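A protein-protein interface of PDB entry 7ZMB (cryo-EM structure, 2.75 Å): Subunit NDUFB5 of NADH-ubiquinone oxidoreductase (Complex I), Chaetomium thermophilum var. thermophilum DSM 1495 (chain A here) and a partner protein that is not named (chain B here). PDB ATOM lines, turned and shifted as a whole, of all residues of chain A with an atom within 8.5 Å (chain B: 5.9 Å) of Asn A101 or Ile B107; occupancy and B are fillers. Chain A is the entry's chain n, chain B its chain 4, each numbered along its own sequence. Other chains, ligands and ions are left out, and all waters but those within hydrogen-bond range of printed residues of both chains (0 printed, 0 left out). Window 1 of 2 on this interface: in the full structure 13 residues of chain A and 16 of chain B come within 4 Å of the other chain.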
ATOM      1  N   TYR A  93     -17.523   9.527 -22.240  1.00  0.00           N
ATOM      2  CA  TYR A  93     -18.681   8.810 -22.767  1.00  0.00           C
ATOM      3  C   TYR A  93     -19.367   9.589 -23.890  1.00  0.00           C
ATOM      4  O   TYR A  93     -20.534   9.975 -23.800  1.00  0.00           O
ATOM      5  CB  TYR A  93     -19.662   8.480 -21.651  1.00  0.00           C
ATOM      6  CG  TYR A  93     -19.027   7.823 -20.445  1.00  0.00           C
ATOM      7  CD1 TYR A  93     -18.803   6.455 -20.417  1.00  0.00           C
ATOM      8  CD2 TYR A  93     -18.661   8.570 -19.334  1.00  0.00           C
ATOM      9  CE1 TYR A  93     -18.235   5.851 -19.316  1.00  0.00           C
ATOM     10  CE2 TYR A  93     -18.095   7.977 -18.236  1.00  0.00           C
ATOM     11  CZ  TYR A  93     -17.886   6.616 -18.229  1.00  0.00           C
ATOM     12  OH  TYR A  93     -17.316   6.017 -17.133  1.00  0.00           O
ATOM     13  N   ASP A  95     -20.265   8.688 -27.023  1.00  0.00           N
ATOM     14  CA  ASP A  95     -21.414   7.956 -27.537  1.00  0.00           C
ATOM     15  C   ASP A  95     -21.501   6.550 -26.960  1.00  0.00           C
ATOM     16  O   ASP A  95     -22.241   5.719 -27.504  1.00  0.00           O
ATOM     17  CB  ASP A  95     -21.374   7.894 -29.068  1.00  0.00           C
ATOM     18  CG  ASP A  95     -19.990   7.588 -29.600  1.00  0.00           C
ATOM     19  OD1 ASP A  95     -19.033   7.576 -28.797  1.00  0.00           O
ATOM     20  OD2 ASP A  95     -19.856   7.361 -30.821  1.00  0.00           O
ATOM     21  N   GLU A  96     -20.769   6.260 -25.884  1.00  0.00           N
ATOM     22  CA  GLU A  96     -20.771   4.918 -25.314  1.00  0.00           C
ATOM     23  C   GLU A  96     -22.160   4.525 -24.832  1.00  0.00           C
ATOM     24  O   GLU A  96     -22.647   3.428 -25.129  1.00  0.00           O
ATOM     25  CB  GLU A  96     -19.763   4.838 -24.168  1.00  0.00           C
ATOM     26  CG  GLU A  96     -19.935   3.626 -23.270  1.00  0.00           C
ATOM     27  CD  GLU A  96     -19.275   2.388 -23.843  1.00  0.00           C
ATOM     28  OE1 GLU A  96     -18.394   2.532 -24.713  1.00  0.00           O
ATOM     29  OE2 GLU A  96     -19.637   1.270 -23.422  1.00  0.00           O
ATOM     30  N   TRP A  97     -22.819   5.415 -24.090  1.00  0.00           N
ATOM     31  CA  TRP A  97     -24.127   5.083 -23.537  1.00  0.00           C
ATOM     32  C   TRP A  97     -25.185   4.977 -24.626  1.00  0.00           C
ATOM     33  O   TRP A  97     -26.055   4.105 -24.565  1.00  0.00           O
ATOM     34  CB  TRP A  97     -24.538   6.118 -22.492  1.00  0.00           C
ATOM     35  CG  TRP A  97     -23.601   6.248 -21.332  1.00  0.00           C
ATOM     36  CD1 TRP A  97     -23.185   7.404 -20.752  1.00  0.00           C
ATOM     37  CD2 TRP A  97     -22.976   5.186 -20.599  1.00  0.00           C
ATOM     38  NE1 TRP A  97     -22.338   7.133 -19.710  1.00  0.00           N
ATOM     39  CE2 TRP A  97     -22.192   5.777 -19.600  1.00  0.00           C
ATOM     40  CE3 TRP A  97     -23.004   3.790 -20.693  1.00  0.00           C
ATOM     41  CZ2 TRP A  97     -21.450   5.028 -18.701  1.00  0.00           C
ATOM     42  CZ3 TRP A  97     -22.267   3.056 -19.810  1.00  0.00           C
ATOM     43  CH2 TRP A  97     -21.494   3.673 -18.831  1.00  0.00           C
ATOM     44  N   GLU A  98     -25.133   5.856 -25.627  1.00  0.00           N
ATOM     45  CA  GLU A  98     -26.160   5.847 -26.661  1.00  0.00           C
ATOM     46  C   GLU A  98     -26.118   4.559 -27.476  1.00  0.00           C
ATOM     47  O   GLU A  98     -27.142   3.893 -27.653  1.00  0.00           O
ATOM     48  CB  GLU A  98     -26.004   7.064 -27.565  1.00  0.00           C
ATOM     49  CG  GLU A  98     -27.149   7.243 -28.539  1.00  0.00           C
ATOM     50  CD  GLU A  98     -26.980   6.390 -29.779  1.00  0.00           C
ATOM     51  OE1 GLU A  98     -25.828   6.180 -30.208  1.00  0.00           O
ATOM     52  OE2 GLU A  98     -27.997   5.883 -30.286  1.00  0.00           O
ATOM     53  N   THR A  99     -24.941   4.192 -27.978  1.00  0.00           N
ATOM     54  CA  THR A  99     -24.832   2.963 -28.749  1.00  0.00           C
ATOM     55  C   THR A  99     -25.215   1.759 -27.905  1.00  0.00           C
ATOM     56  O   THR A  99     -25.900   0.847 -28.383  1.00  0.00           O
ATOM     57  CB  THR A  99     -23.414   2.806 -29.296  1.00  0.00           C
ATOM     58  OG1 THR A  99     -22.478   2.823 -28.211  1.00  0.00           O
ATOM     59  CG2 THR A  99     -23.089   3.942 -30.252  1.00  0.00           C
ATOM     60  N   ARG A 100     -24.778   1.740 -26.643  1.00  0.00           N
ATOM     61  CA  ARG A 100     -25.150   0.654 -25.746  1.00  0.00           C
ATOM     62  C   ARG A 100     -26.652   0.628 -25.503  1.00  0.00           C
ATOM     63  O   ARG A 100     -27.269  -0.442 -25.518  1.00  0.00           O
ATOM     64  CB  ARG A 100     -24.391   0.788 -24.427  1.00  0.00           C
ATOM     65  CG  ARG A 100     -23.109  -0.021 -24.355  1.00  0.00           C
ATOM     66  CD  ARG A 100     -22.532  -0.012 -22.957  1.00  0.00           C
ATOM     67  NE  ARG A 100     -21.476  -1.004 -22.794  1.00  0.00           N
ATOM     68  CZ  ARG A 100     -20.671  -1.069 -21.740  1.00  0.00           C
ATOM     69  NH1 ARG A 100     -20.800  -0.196 -20.750  1.00  0.00           N
ATOM     70  NH2 ARG A 100     -19.735  -2.005 -21.675  1.00  0.00           N
ATOM     71  N   ASN A 101     -27.258   1.793 -25.272  1.00  0.00           N
ATOM     72  CA  ASN A 101     -28.701   1.852 -25.049  1.00  0.00           C
ATOM     73  C   ASN A 101     -29.485   1.399 -26.269  1.00  0.00           C
ATOM     74  O   ASN A 101     -30.479   0.679 -26.137  1.00  0.00           O
ATOM     75  CB  ASN A 101     -29.130   3.267 -24.658  1.00  0.00           C
ATOM     76  CG  ASN A 101     -29.083   3.505 -23.170  1.00  0.00           C
ATOM     77  OD1 ASN A 101     -29.575   2.700 -22.388  1.00  0.00           O
ATOM     78  ND2 ASN A 101     -28.493   4.613 -22.769  1.00  0.00           N
ATOM     79  N   THR A 102     -29.077   1.831 -27.463  1.00  0.00           N
ATOM     80  CA  THR A 102     -29.882   1.542 -28.643  1.00  0.00           C
ATOM     81  C   THR A 102     -29.830   0.060 -29.005  1.00  0.00           C
ATOM     82  O   THR A 102     -30.840  -0.511 -29.428  1.00  0.00           O
ATOM     83  CB  THR A 102     -29.456   2.430 -29.818  1.00  0.00           C
ATOM     84  OG1 THR A 102     -30.368   2.252 -30.908  1.00  0.00           O
ATOM     85  CG2 THR A 102     -28.053   2.119 -30.291  1.00  0.00           C
ATOM     86  N   LEU A 103     -28.676  -0.587 -28.833  1.00  0.00           N
ATOM     87  CA  LEU A 103     -28.622  -2.029 -29.043  1.00  0.00           C
ATOM     88  C   LEU A 103     -29.444  -2.775 -28.006  1.00  0.00           C
ATOM     89  O   LEU A 103     -29.969  -3.857 -28.291  1.00  0.00           O
ATOM     90  CB  LEU A 103     -27.177  -2.530 -29.029  1.00  0.00           C
ATOM     91  CG  LEU A 103     -26.342  -2.471 -30.317  1.00  0.00           C
ATOM     92  CD1 LEU A 103     -26.953  -3.387 -31.364  1.00  0.00           C
ATOM     93  CD2 LEU A 103     -26.198  -1.064 -30.870  1.00  0.00           C
ATOM     94  N   MET A 104     -29.577  -2.221 -26.805  1.00  0.00           N
ATOM     95  CA  MET A 104     -30.365  -2.911 -25.796  1.00  0.00           C
ATOM     96  C   MET A 104     -31.853  -2.797 -26.081  1.00  0.00           C
ATOM     97  O   MET A 104     -32.597  -3.768 -25.911  1.00  0.00           O
ATOM     98  CB  MET A 104     -30.051  -2.370 -24.407  1.00  0.00           C
ATOM     99  CG  MET A 104     -30.729  -3.182 -23.345  1.00  0.00           C
ATOM    100  SD  MET A 104     -30.002  -4.834 -23.378  1.00  0.00           S
ATOM    101  CE  MET A 104     -31.312  -5.814 -22.659  1.00  0.00           C
ATOM    102  N   ALA A 105     -32.306  -1.623 -26.516  1.00  0.00           N
ATOM    103  CA  ALA A 105     -33.721  -1.456 -26.802  1.00  0.00           C
ATOM    104  C   ALA A 105     -34.128  -2.257 -28.027  1.00  0.00           C
ATOM    105  O   ALA A 105     -35.218  -2.836 -28.059  1.00  0.00           O
ATOM    106  CB  ALA A 105     -34.052   0.024 -26.970  1.00  0.00           C
ATOM    107  N   ALA A 106     -33.257  -2.327 -29.034  1.00  0.00           N
ATOM    108  CA  ALA A 106     -33.535  -3.165 -30.195  1.00  0.00           C
ATOM    109  C   ALA A 106     -33.684  -4.629 -29.798  1.00  0.00           C
ATOM    110  O   ALA A 106     -34.603  -5.313 -30.255  1.00  0.00           O
ATOM    111  CB  ALA A 106     -32.424  -3.003 -31.228  1.00  0.00           C
ATOM    112  N   ALA A 107     -32.796  -5.118 -28.938  1.00  0.00           N
ATOM    113  CA  ALA A 107     -32.837  -6.515 -28.530  1.00  0.00           C
ATOM    114  C   ALA A 107     -34.140  -6.857 -27.824  1.00  0.00           C
ATOM    115  O   ALA A 107     -34.638  -7.980 -27.960  1.00  0.00           O
ATOM    116  CB  ALA A 107     -31.642  -6.828 -27.628  1.00  0.00           C
ATOM    117  N   LEU A 108     -34.704  -5.913 -27.073  1.00  0.00           N
ATOM    118  CA  LEU A 108     -35.960  -6.139 -26.371  1.00  0.00           C
ATOM    119  C   LEU A 108     -37.181  -5.808 -27.218  1.00  0.00           C
ATOM    120  O   LEU A 108     -38.242  -6.397 -27.002  1.00  0.00           O
ATOM    121  CB  LEU A 108     -35.983  -5.323 -25.079  1.00  0.00           C
ATOM    122  CG  LEU A 108     -34.837  -5.657 -24.133  1.00  0.00           C
ATOM    123  CD1 LEU A 108     -34.535  -4.474 -23.280  1.00  0.00           C
ATOM    124  CD2 LEU A 108     -35.175  -6.838 -23.267  1.00  0.00           C
ATOM    125  N   SER B   2     -20.524  -3.025 -14.329  1.00  0.00           N
ATOM    126  CA  SER B   2     -21.104  -1.709 -14.100  1.00  0.00           C
ATOM    127  C   SER B   2     -20.944  -1.283 -12.649  1.00  0.00           C
ATOM    128  O   SER B   2     -21.058  -2.097 -11.728  1.00  0.00           O
ATOM    129  CB  SER B   2     -22.582  -1.705 -14.475  1.00  0.00           C
ATOM    130  OG  SER B   2     -23.129  -0.405 -14.352  1.00  0.00           O
ATOM    131  N   LEU B   4     -23.071   0.320 -11.169  1.00  0.00           N
ATOM    132  CA  LEU B   4     -24.396   0.120 -10.605  1.00  0.00           C
ATOM    133  C   LEU B   4     -24.523  -1.252  -9.963  1.00  0.00           C
ATOM    134  O   LEU B   4     -25.166  -1.398  -8.918  1.00  0.00           O
ATOM    135  CB  LEU B   4     -25.450   0.315 -11.694  1.00  0.00           C
ATOM    136  CG  LEU B   4     -26.039   1.721 -11.790  1.00  0.00           C
ATOM    137  CD1 LEU B   4     -24.954   2.758 -11.910  1.00  0.00           C
ATOM    138  CD2 LEU B   4     -26.961   1.806 -12.967  1.00  0.00           C
ATOM    139  N   GLN B 103     -30.062   9.606 -22.573  1.00  0.00           N
ATOM    140  CA  GLN B 103     -29.796   8.147 -22.504  1.00  0.00           C
ATOM    141  C   GLN B 103     -29.537   7.722 -21.058  1.00  0.00           C
ATOM    142  O   GLN B 103     -28.852   8.472 -20.347  1.00  0.00           O
ATOM    143  CB  GLN B 103     -28.511   7.866 -23.285  1.00  0.00           C
ATOM    144  CG  GLN B 103     -28.515   8.419 -24.700  1.00  0.00           C
ATOM    145  CD  GLN B 103     -29.422   7.641 -25.620  1.00  0.00           C
ATOM    146  OE1 GLN B 103     -29.701   6.466 -25.402  1.00  0.00           O
ATOM    147  NE2 GLN B 103     -29.881   8.294 -26.673  1.00  0.00           N
ATOM    148  N   PHE B 104     -30.031   6.559 -20.637  1.00  0.00           N
ATOM    149  CA  PHE B 104     -29.687   6.099 -19.263  1.00  0.00           C
ATOM    150  C   PHE B 104     -28.177   5.835 -19.192  1.00  0.00           C
ATOM    151  O   PHE B 104     -27.620   5.256 -20.143  1.00  0.00           O
ATOM    152  CB  PHE B 104     -30.530   4.890 -18.848  1.00  0.00           C
ATOM    153  CG  PHE B 104     -31.978   5.162 -18.546  1.00  0.00           C
ATOM    154  CD1 PHE B 104     -32.352   5.783 -17.366  1.00  0.00           C
ATOM    155  CD2 PHE B 104     -32.969   4.763 -19.424  1.00  0.00           C
ATOM    156  CE1 PHE B 104     -33.688   6.019 -17.086  1.00  0.00           C
ATOM    157  CE2 PHE B 104     -34.304   5.001 -19.143  1.00  0.00           C
ATOM    158  CZ  PHE B 104     -34.660   5.628 -17.973  1.00  0.00           C
ATOM    159  N   GLN B 105     -27.522   6.257 -18.106  1.00  0.00           N
ATOM    160  CA  GLN B 105     -26.037   6.130 -18.027  1.00  0.00           C
ATOM    161  C   GLN B 105     -25.619   4.955 -17.141  1.00  0.00           C
ATOM    162  O   GLN B 105     -26.437   4.550 -16.300  1.00  0.00           O
ATOM    163  CB  GLN B 105     -25.419   7.440 -17.543  1.00  0.00           C
ATOM    164  CG  GLN B 105     -25.738   8.635 -18.426  1.00  0.00           C
ATOM    165  CD  GLN B 105     -25.257   9.921 -17.803  1.00  0.00           C
ATOM    166  OE1 GLN B 105     -24.264   9.948 -17.083  1.00  0.00           O
ATOM    167  NE2 GLN B 105     -25.965  11.001 -18.078  1.00  0.00           N
ATOM    168  N   PHE B 106     -24.401   4.440 -17.321  1.00  0.00           N
ATOM    169  CA  PHE B 106     -23.862   3.323 -16.546  1.00  0.00           C
ATOM    170  C   PHE B 106     -24.705   2.063 -16.718  1.00  0.00           C
ATOM    171  O   PHE B 106     -24.979   1.336 -15.765  1.00  0.00           O
ATOM    172  CB  PHE B 106     -23.700   3.698 -15.076  1.00  0.00           C
ATOM    173  CG  PHE B 106     -22.950   4.968 -14.875  1.00  0.00           C
ATOM    174  CD1 PHE B 106     -21.594   5.024 -15.110  1.00  0.00           C
ATOM    175  CD2 PHE B 106     -23.608   6.119 -14.485  1.00  0.00           C
ATOM    176  CE1 PHE B 106     -20.901   6.202 -14.947  1.00  0.00           C
ATOM    177  CE2 PHE B 106     -22.923   7.294 -14.324  1.00  0.00           C
ATOM    178  CZ  PHE B 106     -21.564   7.334 -14.553  1.00  0.00           C
ATOM    179  N   ILE B 107     -25.106   1.808 -17.946  1.00  0.00           N
ATOM    180  CA  ILE B 107     -25.771   0.577 -18.342  1.00  0.00           C
ATOM    181  C   ILE B 107     -24.715  -0.432 -18.747  1.00  0.00           C
ATOM    182  O   ILE B 107     -23.578  -0.077 -19.070  1.00  0.00           O
ATOM    183  CB  ILE B 107     -26.756   0.826 -19.496  1.00  0.00           C
ATOM    184  CG1 ILE B 107     -25.983   1.331 -20.708  1.00  0.00           C
ATOM    185  CG2 ILE B 107     -27.833   1.807 -19.077  1.00  0.00           C
ATOM    186  CD1 ILE B 107     -26.788   1.379 -21.950  1.00  0.00           C
ATOM    187  N   GLN B 108     -25.094  -1.705 -18.747  1.00  0.00           N
ATOM    188  CA  GLN B 108     -24.191  -2.793 -19.088  1.00  0.00           C
ATOM    189  C   GLN B 108     -24.815  -3.659 -20.170  1.00  0.00           C
ATOM    190  O   GLN B 108     -26.009  -3.966 -20.120  1.00  0.00           O
ATOM    191  CB  GLN B 108     -23.867  -3.646 -17.857  1.00  0.00           C
ATOM    192  CG  GLN B 108     -22.812  -4.711 -18.085  1.00  0.00           C
ATOM    193  CD  GLN B 108     -22.055  -5.056 -16.819  1.00  0.00           C
ATOM    194  OE1 GLN B 108     -22.441  -4.654 -15.722  1.00  0.00           O
ATOM    195  NE2 GLN B 108     -20.965  -5.803 -16.965  1.00  0.00           N
ATOM    196  N   GLU B 109     -24.001  -4.046 -21.147  1.00  0.00           N
ATOM    197  CA  GLU B 109     -24.447  -4.974 -22.177  1.00  0.00           C
ATOM    198  C   GLU B 109     -24.770  -6.326 -21.558  1.00  0.00           C
ATOM    199  O   GLU B 109     -24.037  -6.814 -20.692  1.00  0.00           O
ATOM    200  CB  GLU B 109     -23.370  -5.132 -23.249  1.00  0.00           C
ATOM    201  CG  GLU B 109     -23.193  -3.923 -24.145  1.00  0.00           C
ATOM    202  CD  GLU B 109     -24.355  -3.734 -25.098  1.00  0.00           C
ATOM    203  OE1 GLU B 109     -24.957  -4.746 -25.512  1.00  0.00           O
ATOM    204  OE2 GLU B 109     -24.661  -2.574 -25.438  1.00  0.00           O
ATOM    205  N   LEU B 120     -29.975  -2.142 -15.248  1.00  0.00           N
ATOM    206  CA  LEU B 120     -29.725  -1.052 -14.318  1.00  0.00           C
ATOM    207  C   LEU B 120     -29.369   0.208 -15.090  1.00  0.00           C
ATOM    208  O   LEU B 120     -28.669   0.147 -16.101  1.00  0.00           O
ATOM    209  CB  LEU B 120     -28.597  -1.406 -13.333  1.00  0.00           C
ATOM    210  CG  LEU B 120     -28.858  -2.510 -12.308  1.00  0.00           C
ATOM    211  CD1 LEU B 120     -27.756  -2.530 -11.278  1.00  0.00           C
ATOM    212  CD2 LEU B 120     -30.201  -2.342 -11.641  1.00  0.00           C
ATOM    213  N   GLY B 121     -29.856   1.345 -14.611  1.00  0.00           N
ATOM    214  CA  GLY B 121     -29.583   2.606 -15.270  1.00  0.00           C
ATOM    215  C   GLY B 121     -29.631   3.751 -14.290  1.00  0.00           C
ATOM    216  O   GLY B 121     -30.263   3.667 -13.233  1.00  0.00           O
ATOM    217  N   VAL B 122     -28.929   4.824 -14.646  1.00  0.00           N
ATOM    218  CA  VAL B 122     -28.888   6.038 -13.783  1.00  0.00           C
ATOM    219  C   VAL B 122     -29.108   7.266 -14.663  1.00  0.00           C
ATOM    220  O   VAL B 122     -28.269   7.527 -15.538  1.00  0.00           O
ATOM    221  CB  VAL B 122     -27.570   6.135 -12.986  1.00  0.00           C
ATOM    222  CG1 VAL B 122     -27.213   7.569 -12.633  1.00  0.00           C
ATOM    223  CG2 VAL B 122     -27.608   5.295 -11.726  1.00  0.00           C
ATOM    224  N   LEU B 173     -34.485  -0.839 -14.815  1.00  0.00           N
ATOM    225  CA  LEU B 173     -34.847  -0.142 -16.043  1.00  0.00           C
ATOM    226  C   LEU B 173     -36.101  -0.704 -16.708  1.00  0.00           C
ATOM    227  O   LEU B 173     -36.267  -0.573 -17.918  1.00  0.00           O
ATOM    228  CB  LEU B 173     -33.682  -0.162 -17.028  1.00  0.00           C
ATOM    229  CG  LEU B 173     -32.522   0.775 -16.722  1.00  0.00           C
ATOM    230  CD1 LEU B 173     -31.563   0.808 -17.886  1.00  0.00           C
ATOM    231  CD2 LEU B 173     -33.052   2.157 -16.422  1.00  0.00           C
ATOM    232  N   TYR B 234     -39.501  -2.674 -20.494  1.00  0.00           N
ATOM    233  CA  TYR B 234     -38.274  -1.892 -20.563  1.00  0.00           C
ATOM    234  C   TYR B 234     -38.594  -0.422 -20.777  1.00  0.00           C
ATOM    235  O   TYR B 234     -39.402  -0.079 -21.643  1.00  0.00           O
ATOM    236  CB  TYR B 234     -37.393  -2.424 -21.696  1.00  0.00           C
ATOM    237  CG  TYR B 234     -35.985  -1.874 -21.709  1.00  0.00           C
ATOM    238  CD1 TYR B 234     -35.081  -2.194 -20.703  1.00  0.00           C
ATOM    239  CD2 TYR B 234     -35.557  -1.045 -22.731  1.00  0.00           C
ATOM    240  CE1 TYR B 234     -33.804  -1.699 -20.717  1.00  0.00           C
ATOM    241  CE2 TYR B 234     -34.282  -0.545 -22.751  1.00  0.00           C
ATOM    242  CZ  TYR B 234     -33.409  -0.870 -21.741  1.00  0.00           C
ATOM    243  OH  TYR B 234     -32.133  -0.365 -21.768  1.00  0.00           O
ATOM    244  N   ASP B 236     -37.187   2.213 -22.083  1.00  0.00           N
ATOM    245  CA  ASP B 236     -37.017   2.840 -23.388  1.00  0.00           C
ATOM    246  C   ASP B 236     -38.108   2.425 -24.363  1.00  0.00           C
ATOM    247  O   ASP B 236     -38.648   3.267 -25.083  1.00  0.00           O
ATOM    248  CB  ASP B 236     -35.637   2.509 -23.947  1.00  0.00           C
ATOM    249  CG  ASP B 236     -34.549   3.364 -23.330  1.00  0.00           C
ATOM    250  OD1 ASP B 236     -34.890   4.385 -22.700  1.00  0.00           O
ATOM    251  OD2 ASP B 236     -33.357   3.019 -23.473  1.00  0.00           O
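OE1 of Gln B103 sits close to ND2 of Asn A101, 3.4 Å away. The backbone carbonyl oxygen (O) of Phe B104 sits at hydrogen-bond distance from the side-chain amide nitrogen (ND2) of Asn A101, 2.8 Å away. The backbone carbonyl oxygen (O) of Ile B107 sits at hydrogen-bond distance from the guanidinium group (NH1) of Arg A100 (3.2 Å). O of Arg A100 lies close to OE2 of Glu B109 (3.4 Å).
The backbone carbonyl oxygen (O) of Phe B106 lies within hydrogen-bond range of the side-chain hydroxyl (OG) of Ser B2, 2.9 Å away. N of Gln B105 sits at hydrogen-bond distance from O of Val B122 (3.0 Å). The side-chain carboxylate of Glu A96 lies within salt-bridge range of the guanidinium group of Arg A100, at 3.0 Å. The backbone carbonyl oxygen of Trp A97 lies within hydrogen-bond range of the side-chain amide nitrogen of Asn A101, at 3.1 Å.
Among the printed residues, merely in contact across the chains: Trp A97 with Phe B104, Trp A97 with Gln B105, Trp A97 with Phe B106, Trp A97 with Ile B107, Glu A98 with Gln B103, Asn A101 with Ile B107, Asn A101 with Asp B236, Met A104 with Tyr B234 and Leu A108 with Tyr B234.
Ile B107 touches three residues of chain A. Of the printed residues of chain A, Glu B109 touches Arg A100 (3.2 Å). Of the printed residues of chain A, Tyr B234 touches Met A104 (3.5 Å) and Leu A108 (3.4 Å). Ala A106 touches none of the printed residues of chain B. The nearest residue of chain B that does not touch Asn A101 is Tyr B234 (4.04 Å). The nearest printed residue of chain B that does not touch Met A104 is Glu B109 (5.1 Å).
Of the 15 printed residues of chain A, 6 touch a printed residue of chain B. Hydrophobic or aromatic side chains of chain A within 4 Å of the printed part of chain B: Trp A97, Met A104 and Leu A108. Printed residues of chain B that touch a printed residue of chain A: Gln B103, Phe B104, Gln B105, Phe B106, Ile B107, Glu B109, Tyr B234 and Asp B236.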
